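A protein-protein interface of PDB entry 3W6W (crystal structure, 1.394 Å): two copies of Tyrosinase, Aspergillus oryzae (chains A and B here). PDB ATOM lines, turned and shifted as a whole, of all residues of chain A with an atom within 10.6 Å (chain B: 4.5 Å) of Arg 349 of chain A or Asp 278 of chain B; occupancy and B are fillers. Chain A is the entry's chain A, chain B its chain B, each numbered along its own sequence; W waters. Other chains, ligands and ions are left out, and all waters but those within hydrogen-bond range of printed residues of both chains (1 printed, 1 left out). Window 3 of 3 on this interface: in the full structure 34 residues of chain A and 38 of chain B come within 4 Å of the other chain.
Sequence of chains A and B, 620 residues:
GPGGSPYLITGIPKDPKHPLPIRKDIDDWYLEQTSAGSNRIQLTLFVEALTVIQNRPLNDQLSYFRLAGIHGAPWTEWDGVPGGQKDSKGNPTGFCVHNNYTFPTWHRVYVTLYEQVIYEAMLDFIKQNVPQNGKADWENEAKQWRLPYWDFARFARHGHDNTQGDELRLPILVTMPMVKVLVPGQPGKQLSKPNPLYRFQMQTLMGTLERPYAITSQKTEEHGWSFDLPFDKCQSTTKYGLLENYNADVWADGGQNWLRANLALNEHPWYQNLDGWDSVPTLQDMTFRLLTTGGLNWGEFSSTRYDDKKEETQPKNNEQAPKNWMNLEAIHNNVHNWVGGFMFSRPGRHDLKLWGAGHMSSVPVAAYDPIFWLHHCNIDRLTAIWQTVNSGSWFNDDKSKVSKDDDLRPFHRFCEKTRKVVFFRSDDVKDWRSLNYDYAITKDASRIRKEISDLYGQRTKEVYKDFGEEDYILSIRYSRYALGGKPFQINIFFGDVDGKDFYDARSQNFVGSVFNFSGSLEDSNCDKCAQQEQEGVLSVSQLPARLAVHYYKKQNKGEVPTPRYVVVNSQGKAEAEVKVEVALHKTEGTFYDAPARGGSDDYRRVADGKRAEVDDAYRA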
ATOM      1  N   ASN A 245     -15.245 -18.810   9.878  1.00  0.00           N
ATOM      2  CA  ASN A 245     -16.510 -19.486  10.198  1.00  0.00           C
ATOM      3  C   ASN A 245     -17.612 -18.536  10.637  1.00  0.00           C
ATOM      4  O   ASN A 245     -18.542 -18.929  11.341  1.00  0.00           O
ATOM      5  CB  ASN A 245     -16.345 -20.601  11.239  1.00  0.00           C
ATOM      6  CG  ASN A 245     -15.507 -21.759  10.734  1.00  0.00           C
ATOM      7  OD1 ASN A 245     -15.563 -22.127   9.557  1.00  0.00           O
ATOM      8  ND2 ASN A 245     -14.716 -22.332  11.625  1.00  0.00           N
ATOM      9  N   SER A 345      -8.217 -17.951  13.190  1.00  0.00           N
ATOM     10  CA  SER A 345      -8.921 -19.158  13.589  1.00  0.00           C
ATOM     11  C   SER A 345      -8.215 -19.873  14.733  1.00  0.00           C
ATOM     12  O   SER A 345      -7.096 -19.520  15.089  1.00  0.00           O
ATOM     13  CB  SER A 345      -9.039 -20.089  12.385  1.00  0.00           C
ATOM     14  OG  SER A 345     -10.011 -21.085  12.622  1.00  0.00           O
ATOM     15  N   ARG A 346      -8.888 -20.880  15.278  1.00  0.00           N
ATOM     16  CA  ARG A 346      -8.305 -21.786  16.261  1.00  0.00           C
ATOM     17  C   ARG A 346      -8.880 -23.169  15.993  1.00  0.00           C
ATOM     18  O   ARG A 346     -10.072 -23.297  15.701  1.00  0.00           O
ATOM     19  CB  ARG A 346      -8.639 -21.352  17.690  1.00  0.00           C
ATOM     20  CG  ARG A 346      -7.843 -22.145  18.732  1.00  0.00           C
ATOM     21  CD  ARG A 346      -7.836 -21.475  20.095  1.00  0.00           C
ATOM     22  NE  ARG A 346      -7.218 -20.156  20.046  1.00  0.00           N
ATOM     23  CZ  ARG A 346      -7.041 -19.362  21.100  1.00  0.00           C
ATOM     24  NH1 ARG A 346      -7.418 -19.770  22.307  1.00  0.00           N
ATOM     25  NH2 ARG A 346      -6.488 -18.169  20.956  1.00  0.00           N
ATOM     26  N   PRO A 347      -8.048 -24.214  16.082  1.00  0.00           N
ATOM     27  CA  PRO A 347      -8.582 -25.565  15.896  1.00  0.00           C
ATOM     28  C   PRO A 347      -9.504 -25.967  17.048  1.00  0.00           C
ATOM     29  O   PRO A 347      -9.454 -25.347  18.110  1.00  0.00           O
ATOM     30  CB  PRO A 347      -7.322 -26.436  15.910  1.00  0.00           C
ATOM     31  CG  PRO A 347      -6.224 -25.530  15.520  1.00  0.00           C
ATOM     32  CD  PRO A 347      -6.574 -24.209  16.134  1.00  0.00           C
ATOM     33  N   GLY A 348     -10.354 -26.957  16.817  1.00  0.00           N
ATOM     34  CA  GLY A 348     -11.114 -27.586  17.889  1.00  0.00           C
ATOM     35  C   GLY A 348     -12.288 -26.820  18.477  1.00  0.00           C
ATOM     36  O   GLY A 348     -12.852 -25.936  17.845  1.00  0.00           O
ATOM     37  N   ARG A 349     -12.652 -27.181  19.703  1.00  0.00           N
ATOM     38  CA  ARG A 349     -13.841 -26.652  20.372  1.00  0.00           C
ATOM     39  C   ARG A 349     -13.477 -25.628  21.433  1.00  0.00           C
ATOM     40  O   ARG A 349     -12.719 -25.934  22.355  1.00  0.00           O
ATOM     41  CB  ARG A 349     -14.614 -27.791  21.046  1.00  0.00           C
ATOM     42  CG  ARG A 349     -15.564 -27.316  22.145  1.00  0.00           C
ATOM     43  CD  ARG A 349     -16.127 -28.462  22.975  1.00  0.00           C
ATOM     44  NE  ARG A 349     -15.221 -28.948  24.022  1.00  0.00           N
ATOM     45  CZ  ARG A 349     -15.637 -29.589  25.113  1.00  0.00           C
ATOM     46  NH1 ARG A 349     -16.935 -29.805  25.287  1.00  0.00           N
ATOM     47  NH2 ARG A 349     -14.769 -30.017  26.029  1.00  0.00           N
ATOM     48  N   HIS A 350     -14.004 -24.409  21.299  1.00  0.00           N
ATOM     49  CA  HIS A 350     -13.784 -23.359  22.293  1.00  0.00           C
ATOM     50  C   HIS A 350     -14.995 -22.436  22.377  1.00  0.00           C
ATOM     51  O   HIS A 350     -15.327 -21.772  21.397  1.00  0.00           O
ATOM     52  CB  HIS A 350     -12.539 -22.529  21.938  1.00  0.00           C
ATOM     53  CG  HIS A 350     -11.324 -23.356  21.664  1.00  0.00           C
ATOM     54  ND1 HIS A 350     -10.511 -23.837  22.668  1.00  0.00           N
ATOM     55  CD2 HIS A 350     -10.809 -23.828  20.503  1.00  0.00           C
ATOM     56  CE1 HIS A 350      -9.535 -24.553  22.135  1.00  0.00           C
ATOM     57  NE2 HIS A 350      -9.698 -24.566  20.823  1.00  0.00           N
ATOM     58  N   ASP A 351     -15.663 -22.379  23.529  1.00  0.00           N
ATOM     59  CA  ASP A 351     -16.792 -21.468  23.688  1.00  0.00           C
ATOM     60  C   ASP A 351     -16.316 -20.028  23.822  1.00  0.00           C
ATOM     61  O   ASP A 351     -16.803 -19.145  23.130  1.00  0.00           O
ATOM     62  CB  ASP A 351     -17.638 -21.852  24.895  1.00  0.00           C
ATOM     63  CG  ASP A 351     -18.436 -23.112  24.664  1.00  0.00           C
ATOM     64  OD1 ASP A 351     -19.042 -23.242  23.579  1.00  0.00           O
ATOM     65  OD2 ASP A 351     -18.447 -23.970  25.561  1.00  0.00           O
ATOM     66  N   LEU A 352     -15.343 -19.801  24.703  1.00  0.00           N
ATOM     67  CA  LEU A 352     -14.722 -18.476  24.809  1.00  0.00           C
ATOM     68  C   LEU A 352     -13.711 -18.352  23.692  1.00  0.00           C
ATOM     69  O   LEU A 352     -12.752 -19.118  23.624  1.00  0.00           O
ATOM     70  CB  LEU A 352     -14.049 -18.267  26.170  1.00  0.00           C
ATOM     71  CG  LEU A 352     -13.177 -17.014  26.317  1.00  0.00           C
ATOM     72  CD1 LEU A 352     -13.993 -15.746  26.148  1.00  0.00           C
ATOM     73  CD2 LEU A 352     -12.450 -17.023  27.654  1.00  0.00           C
ATOM     74  N   LYS A 353     -13.950 -17.397  22.812  1.00  0.00           N
ATOM     75  CA  LYS A 353     -13.107 -17.229  21.645  1.00  0.00           C
ATOM     76  C   LYS A 353     -12.215 -16.005  21.819  1.00  0.00           C
ATOM     77  O   LYS A 353     -12.679 -14.864  21.847  1.00  0.00           O
ATOM     78  CB  LYS A 353     -13.977 -17.158  20.390  1.00  0.00           C
ATOM     79  CG  LYS A 353     -14.878 -18.387  20.242  1.00  0.00           C
ATOM     80  CD  LYS A 353     -15.867 -18.240  19.103  1.00  0.00           C
ATOM     81  CE  LYS A 353     -16.896 -19.355  19.100  1.00  0.00           C
ATOM     82  NZ  LYS A 353     -16.290 -20.694  18.958  1.00  0.00           N
ATOM     83  N   LEU A 354     -10.918 -16.262  21.941  1.00  0.00           N
ATOM     84  CA  LEU A 354      -9.962 -15.213  22.254  1.00  0.00           C
ATOM     85  C   LEU A 354      -9.170 -14.793  21.030  1.00  0.00           C
ATOM     86  O   LEU A 354      -8.377 -13.853  21.095  1.00  0.00           O
ATOM     87  CB  LEU A 354      -9.027 -15.694  23.363  1.00  0.00           C
ATOM     88  CG  LEU A 354      -9.749 -15.918  24.691  1.00  0.00           C
ATOM     89  CD1 LEU A 354      -8.966 -16.854  25.615  1.00  0.00           C
ATOM     90  CD2 LEU A 354      -9.991 -14.581  25.341  1.00  0.00           C
ATOM     91  N   TRP A 355      -9.401 -15.479  19.917  1.00  0.00           N
ATOM     92  CA  TRP A 355      -8.737 -15.123  18.665  1.00  0.00           C
ATOM     93  C   TRP A 355      -9.554 -14.100  17.900  1.00  0.00           C
ATOM     94  O   TRP A 355     -10.512 -13.553  18.427  1.00  0.00           O
ATOM     95  CB  TRP A 355      -8.453 -16.366  17.805  1.00  0.00           C
ATOM     96  CG  TRP A 355      -9.650 -17.134  17.328  1.00  0.00           C
ATOM     97  CD1 TRP A 355     -10.251 -17.041  16.105  1.00  0.00           C
ATOM     98  CD2 TRP A 355     -10.382 -18.128  18.061  1.00  0.00           C
ATOM     99  NE1 TRP A 355     -11.308 -17.916  16.025  1.00  0.00           N
ATOM    100  CE2 TRP A 355     -11.409 -18.600  17.213  1.00  0.00           C
ATOM    101  CE3 TRP A 355     -10.256 -18.679  19.342  1.00  0.00           C
ATOM    102  CZ2 TRP A 355     -12.312 -19.583  17.609  1.00  0.00           C
ATOM    103  CZ3 TRP A 355     -11.153 -19.655  19.734  1.00  0.00           C
ATOM    104  CH2 TRP A 355     -12.164 -20.106  18.871  1.00  0.00           C
ATOM    105  N   ASP A 498      -0.160 -27.087  27.680  1.00  0.00           N
ATOM    106  CA  ASP A 498      -1.468 -27.618  27.329  1.00  0.00           C
ATOM    107  C   ASP A 498      -1.512 -27.711  25.807  1.00  0.00           C
ATOM    108  O   ASP A 498      -1.399 -26.704  25.113  1.00  0.00           O
ATOM    109  CB  ASP A 498      -2.542 -26.655  27.861  1.00  0.00           C
ATOM    110  CG  ASP A 498      -3.966 -27.130  27.611  1.00  0.00           C
ATOM    111  OD1 ASP A 498      -4.219 -27.927  26.678  1.00  0.00           O
ATOM    112  OD2 ASP A 498      -4.854 -26.670  28.367  1.00  0.00           O
ATOM    113  N   GLY A 499      -1.666 -28.922  25.285  1.00  0.00           N
ATOM    114  CA  GLY A 499      -1.612 -29.143  23.851  1.00  0.00           C
ATOM    115  C   GLY A 499      -2.762 -28.569  23.051  1.00  0.00           C
ATOM    116  O   GLY A 499      -2.738 -28.637  21.829  1.00  0.00           O
ATOM    117  N   LYS A 500      -3.768 -28.030  23.735  1.00  0.00           N
ATOM    118  CA  LYS A 500      -4.904 -27.368  23.088  1.00  0.00           C
ATOM    119  C   LYS A 500      -5.027 -25.905  23.502  1.00  0.00           C
ATOM    120  O   LYS A 500      -6.017 -25.250  23.177  1.00  0.00           O
ATOM    121  CB  LYS A 500      -6.214 -28.081  23.433  1.00  0.00           C
ATOM    122  CG  LYS A 500      -6.269 -29.543  23.025  1.00  0.00           C
ATOM    123  CD  LYS A 500      -7.639 -30.129  23.335  1.00  0.00           C
ATOM    124  CE  LYS A 500      -7.551 -31.212  24.389  1.00  0.00           C
ATOM    125  NZ  LYS A 500      -6.724 -32.339  23.970  1.00  0.00           N
ATOM    126  N   ASP A 501      -4.032 -25.391  24.215  1.00  0.00           N
ATOM    127  CA  ASP A 501      -4.115 -24.031  24.732  1.00  0.00           C
ATOM    128  C   ASP A 501      -2.722 -23.482  25.011  1.00  0.00           C
ATOM    129  O   ASP A 501      -2.204 -23.611  26.121  1.00  0.00           O
ATOM    130  CB  ASP A 501      -4.955 -24.011  26.012  1.00  0.00           C
ATOM    131  CG  ASP A 501      -5.366 -22.604  26.423  1.00  0.00           C
ATOM    132  OD1 ASP A 501      -4.981 -21.619  25.757  1.00  0.00           O
ATOM    133  OD2 ASP A 501      -6.066 -22.476  27.450  1.00  0.00           O
ATOM    134  N   TYR A 503      -1.493 -20.177  23.819  1.00  0.00           N
ATOM    135  CA  TYR A 503      -1.741 -18.941  23.083  1.00  0.00           C
ATOM    136  C   TYR A 503      -1.498 -17.621  23.798  1.00  0.00           C
ATOM    137  O   TYR A 503      -1.103 -16.636  23.163  1.00  0.00           O
ATOM    138  CB  TYR A 503      -3.197 -18.915  22.617  1.00  0.00           C
ATOM    139  CG  TYR A 503      -3.550 -20.052  21.701  1.00  0.00           C
ATOM    140  CD1 TYR A 503      -3.087 -20.068  20.393  1.00  0.00           C
ATOM    141  CD2 TYR A 503      -4.326 -21.111  22.138  1.00  0.00           C
ATOM    142  CE1 TYR A 503      -3.393 -21.107  19.547  1.00  0.00           C
ATOM    143  CE2 TYR A 503      -4.645 -22.162  21.303  1.00  0.00           C
ATOM    144  CZ  TYR A 503      -4.179 -22.149  19.999  1.00  0.00           C
ATOM    145  OH  TYR A 503      -4.506 -23.187  19.154  1.00  0.00           O
ATOM    146  N   ASP A 615      -1.106 -30.835  20.703  1.00  0.00           N
ATOM    147  CA  ASP A 615      -1.981 -31.906  20.230  1.00  0.00           C
ATOM    148  C   ASP A 615      -1.894 -32.015  18.716  1.00  0.00           C
ATOM    149  O   ASP A 615      -1.736 -31.016  18.022  1.00  0.00           O
ATOM    150  CB  ASP A 615      -3.434 -31.643  20.622  1.00  0.00           C
ATOM    151  CG  ASP A 615      -3.767 -32.126  22.013  1.00  0.00           C
ATOM    152  OD1 ASP A 615      -2.847 -32.260  22.856  1.00  0.00           O
ATOM    153  OD2 ASP A 615      -4.967 -32.373  22.264  1.00  0.00           O
ATOM    154  N   ALA A 617      -4.023 -32.389  16.416  1.00  0.00           N
ATOM    155  CA  ALA A 617      -4.994 -31.566  15.696  1.00  0.00           C
ATOM    156  C   ALA A 617      -4.626 -30.086  15.674  1.00  0.00           C
ATOM    157  O   ALA A 617      -5.199 -29.309  14.905  1.00  0.00           O
ATOM    158  CB  ALA A 617      -6.380 -31.750  16.280  1.00  0.00           C
ATOM    159  N   TYR A 618      -3.668 -29.703  16.509  1.00  0.00           N
ATOM    160  CA  TYR A 618      -3.248 -28.312  16.608  1.00  0.00           C
ATOM    161  C   TYR A 618      -1.891 -28.077  15.940  1.00  0.00           C
ATOM    162  O   TYR A 618      -1.327 -26.984  16.032  1.00  0.00           O
ATOM    163  CB  TYR A 618      -3.202 -27.876  18.080  1.00  0.00           C
ATOM    164  CG  TYR A 618      -4.560 -27.668  18.716  1.00  0.00           C
ATOM    165  CD1 TYR A 618      -5.397 -28.743  18.999  1.00  0.00           C
ATOM    166  CD2 TYR A 618      -5.000 -26.392  19.054  1.00  0.00           C
ATOM    167  CE1 TYR A 618      -6.644 -28.551  19.587  1.00  0.00           C
ATOM    168  CE2 TYR A 618      -6.233 -26.191  19.630  1.00  0.00           C
ATOM    169  CZ  TYR A 618      -7.053 -27.267  19.899  1.00  0.00           C
ATOM    170  OH  TYR A 618      -8.283 -27.070  20.477  1.00  0.00           O
ATOM    171  N   GLN B 272     -18.190 -28.957  31.446  1.00  0.00           N
ATOM    172  CA  GLN B 272     -18.142 -29.303  30.027  1.00  0.00           C
ATOM    173  C   GLN B 272     -16.996 -28.646  29.285  1.00  0.00           C
ATOM    174  O   GLN B 272     -16.664 -29.074  28.180  1.00  0.00           O
ATOM    175  CB  GLN B 272     -19.478 -29.034  29.339  1.00  0.00           C
ATOM    176  CG  GLN B 272     -20.570 -29.970  29.844  1.00  0.00           C
ATOM    177  CD  GLN B 272     -21.966 -29.612  29.359  1.00  0.00           C
ATOM    178  OE1 GLN B 272     -22.162 -28.644  28.620  1.00  0.00           O
ATOM    179  NE2 GLN B 272     -22.951 -30.394  29.796  1.00  0.00           N
ATOM    180  N   ASN B 273     -16.374 -27.633  29.880  1.00  0.00           N
ATOM    181  CA  ASN B 273     -15.160 -27.079  29.282  1.00  0.00           C
ATOM    182  C   ASN B 273     -13.891 -27.855  29.625  1.00  0.00           C
ATOM    183  O   ASN B 273     -12.822 -27.530  29.113  1.00  0.00           O
ATOM    184  CB  ASN B 273     -14.990 -25.609  29.629  1.00  0.00           C
ATOM    185  CG  ASN B 273     -16.048 -24.748  28.989  1.00  0.00           C
ATOM    186  OD1 ASN B 273     -16.504 -25.033  27.876  1.00  0.00           O
ATOM    187  ND2 ASN B 273     -16.456 -23.702  29.686  1.00  0.00           N
ATOM    188  N   LEU B 274     -14.011 -28.861  30.491  1.00  0.00           N
ATOM    189  CA  LEU B 274     -12.893 -29.735  30.817  1.00  0.00           C
ATOM    190  C   LEU B 274     -12.715 -30.730  29.686  1.00  0.00           C
ATOM    191  O   LEU B 274     -13.674 -31.082  29.000  1.00  0.00           O
ATOM    192  CB  LEU B 274     -13.151 -30.484  32.126  1.00  0.00           C
ATOM    193  CG  LEU B 274     -13.370 -29.609  33.363  1.00  0.00           C
ATOM    194  CD1 LEU B 274     -13.827 -30.450  34.532  1.00  0.00           C
ATOM    195  CD2 LEU B 274     -12.096 -28.857  33.717  1.00  0.00           C
ATOM    196  N   GLY B 276     -12.480 -33.859  27.359  1.00  0.00           N
ATOM    197  CA  GLY B 276     -13.130 -35.153  27.287  1.00  0.00           C
ATOM    198  C   GLY B 276     -14.650 -35.152  27.340  1.00  0.00           C
ATOM    199  O   GLY B 276     -15.286 -36.132  26.951  1.00  0.00           O
ATOM    200  N   TRP B 277     -15.236 -34.073  27.839  1.00  0.00           N
ATOM    201  CA  TRP B 277     -16.687 -33.977  27.957  1.00  0.00           C
ATOM    202  C   TRP B 277     -17.318 -33.285  26.758  1.00  0.00           C
ATOM    203  O   TRP B 277     -16.728 -32.361  26.200  1.00  0.00           O
ATOM    204  CB  TRP B 277     -17.038 -33.219  29.231  1.00  0.00           C
ATOM    205  CG  TRP B 277     -16.539 -33.870  30.470  1.00  0.00           C
ATOM    206  CD1 TRP B 277     -15.444 -33.512  31.201  1.00  0.00           C
ATOM    207  CD2 TRP B 277     -17.111 -35.001  31.130  1.00  0.00           C
ATOM    208  NE1 TRP B 277     -15.309 -34.340  32.285  1.00  0.00           N
ATOM    209  CE2 TRP B 277     -16.314 -35.274  32.260  1.00  0.00           C
ATOM    210  CE3 TRP B 277     -18.223 -35.812  30.878  1.00  0.00           C
ATOM    211  CZ2 TRP B 277     -16.605 -36.307  33.141  1.00  0.00           C
ATOM    212  CZ3 TRP B 277     -18.506 -36.843  31.753  1.00  0.00           C
ATOM    213  CH2 TRP B 277     -17.695 -37.087  32.865  1.00  0.00           C
ATOM    214  N   ASP B 278     -18.514 -33.732  26.369  1.00  0.00           N
ATOM    215  CA  ASP B 278     -19.295 -33.067  25.321  1.00  0.00           C
ATOM    216  C   ASP B 278     -20.161 -31.967  25.933  1.00  0.00           C
ATOM    217  O   ASP B 278     -20.674 -32.116  27.036  1.00  0.00           O
ATOM    218  CB  ASP B 278     -20.193 -34.066  24.581  1.00  0.00           C
ATOM    219  CG  ASP B 278     -19.409 -35.003  23.675  1.00  0.00           C
ATOM    220  OD1 ASP B 278     -18.369 -34.566  23.141  1.00  0.00           O
ATOM    221  OD2 ASP B 278     -19.825 -36.166  23.493  1.00  0.00           O
ATOM    222  N   SER B 279     -20.340 -30.867  25.217  1.00  0.00           N
ATOM    223  CA  SER B 279     -21.179 -29.802  25.755  1.00  0.00           C
ATOM    224  C   SER B 279     -22.566 -29.802  25.120  1.00  0.00           C
ATOM    225  O   SER B 279     -22.756 -30.281  24.006  1.00  0.00           O
ATOM    226  CB  SER B 279     -20.518 -28.432  25.582  1.00  0.00           C
ATOM    227  OG  SER B 279     -20.529 -28.041  24.223  1.00  0.00           O
ATOM    228  N   VAL B 280     -23.536 -29.261  25.856  1.00  0.00           N
ATOM    229  CA  VAL B 280     -24.896 -29.072  25.365  1.00  0.00           C
ATOM    230  C   VAL B 280     -25.280 -27.663  25.808  1.00  0.00           C
ATOM    231  O   VAL B 280     -25.206 -27.366  27.000  1.00  0.00           O
ATOM    232  CB  VAL B 280     -25.889 -30.078  26.021  1.00  0.00           C
ATOM    233  CG1 VAL B 280     -27.323 -29.824  25.532  1.00  0.00           C
ATOM    234  CG2 VAL B 280     -25.458 -31.528  25.782  1.00  0.00           C
ATOM    235  N   ARG B 459     -28.709 -32.786  19.909  1.00  0.00           N
ATOM    236  CA  ARG B 459     -27.510 -32.701  20.734  1.00  0.00           C
ATOM    237  C   ARG B 459     -27.753 -33.171  22.161  1.00  0.00           C
ATOM    238  O   ARG B 459     -26.915 -33.870  22.743  1.00  0.00           O
ATOM    239  CB  ARG B 459     -26.949 -31.283  20.725  1.00  0.00           C
ATOM    240  CG  ARG B 459     -25.640 -31.128  21.478  1.00  0.00           C
ATOM    241  CD  ARG B 459     -24.554 -32.068  20.949  1.00  0.00           C
ATOM    242  NE  ARG B 459     -23.261 -31.705  21.518  1.00  0.00           N
ATOM    243  CZ  ARG B 459     -22.127 -32.363  21.328  1.00  0.00           C
ATOM    244  NH1 ARG B 459     -21.018 -31.924  21.905  1.00  0.00           N
ATOM    245  NH2 ARG B 459     -22.101 -33.456  20.572  1.00  0.00           N
ATOM    246  N   VAL B 463     -25.765 -36.543  23.736  1.00  0.00           N
ATOM    247  CA  VAL B 463     -24.909 -36.464  24.911  1.00  0.00           C
ATOM    248  C   VAL B 463     -25.492 -37.204  26.122  1.00  0.00           C
ATOM    249  O   VAL B 463     -24.766 -37.885  26.839  1.00  0.00           O
ATOM    250  CB  VAL B 463     -24.580 -35.003  25.262  1.00  0.00           C
ATOM    251  CG1 VAL B 463     -23.794 -34.922  26.563  1.00  0.00           C
ATOM    252  CG2 VAL B 463     -23.803 -34.356  24.116  1.00  0.00           C
HETATM  253  O   HOH W   1     -15.181 -24.399  25.437  1.00  0.00           O
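Among the printed residues, merely in contact across the chains: Arg 349 of chain A with Asp 278 of chain B (3.9 Å) and Arg 349 of chain A with Ser 279 of chain B (3.6 Å).
No position is printed for both chains.
The side-chain carboxylate of Asp 278 of chain B is in salt-bridge range of the guanidinium group of Arg 459 of chain B.
N of Val 280 of chain B is in hydrogen-bond range of OE1 of Gln 272 of chain B.
The backbone carbonyl oxygen (O) of Ser 279 of chain B is in hydrogen-bond range of the guanidinium group (NE) of Arg 459 of chain B.
Water W1 bridges the backbone NH (N) of Asp 351 of chain A (2.8 Å) and the side-chain amide oxygen (OD1) of Asn 273 of chain B (2.8 Å).
Of the 10 printed residues of chain B, 6 touch a printed residue of chain A.
Among the printed residues, 6 pairs touch across the chains.
The guanidinium group (NH2) of Arg 349 of chain A lies within hydrogen-bond range of the backbone carbonyl oxygen (O) of Leu 274 of chain B, at 3.3 Å.
The guanidinium group (NH1) of Arg 349 of chain A lies within hydrogen-bond range of the backbone carbonyl oxygen (O) of Trp 277 of chain B.
NH1 of Arg 349 of chain A sits at hydrogen-bond distance from O of Gln 272 of chain B (3.0 Å).
The side-chain carboxylate (OD2) of Asp 351 of chain A sits close to the side-chain amide oxygen (OD1) of Asn 273 of chain B (3.2 Å).
Arg 349 of chain A touches just these residues of chain B: Gln 272 (3.0 Å), Leu 274 (3.3 Å), Trp 277 (2.7 Å), Asp 278 (3.9 Å) and Ser 279 (3.6 Å).
Tyr 503 of chain A touches none of the printed residues of chain B.
Of chain A, only Arg 349 (3.0 Å) comes within 4 Å of Gln 272 of chain B.
Printed residues of chain A within 4 Å of Asn 273 of chain B: Asp 351.
Of the printed residues of chain A, Leu 274 of chain B touches Arg 349.
No residue of chain A comes within 4 Å of Gly 276 of chain B.
Of the printed residues of chain A, Trp 277 of chain B touches Arg 349 (2.7 Å).
Of the printed residues of chain A, Ser 279 of chain B touches Arg 349 (3.6 Å).
Arg 459 of chain B touches none of the printed residues of chain A.
The nearest residue of chain B that does not touch Arg 349 of chain A is Asn 273 of chain B (4.3 Å).
The nearest printed residue of chain A that does not touch Asp 278 of chain B is Asp 351 of chain A (8.2 Å).
The nearest printed residue of chain A that does not touch Leu 274 of chain B is Lys 500 of chain A (7.4 Å).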
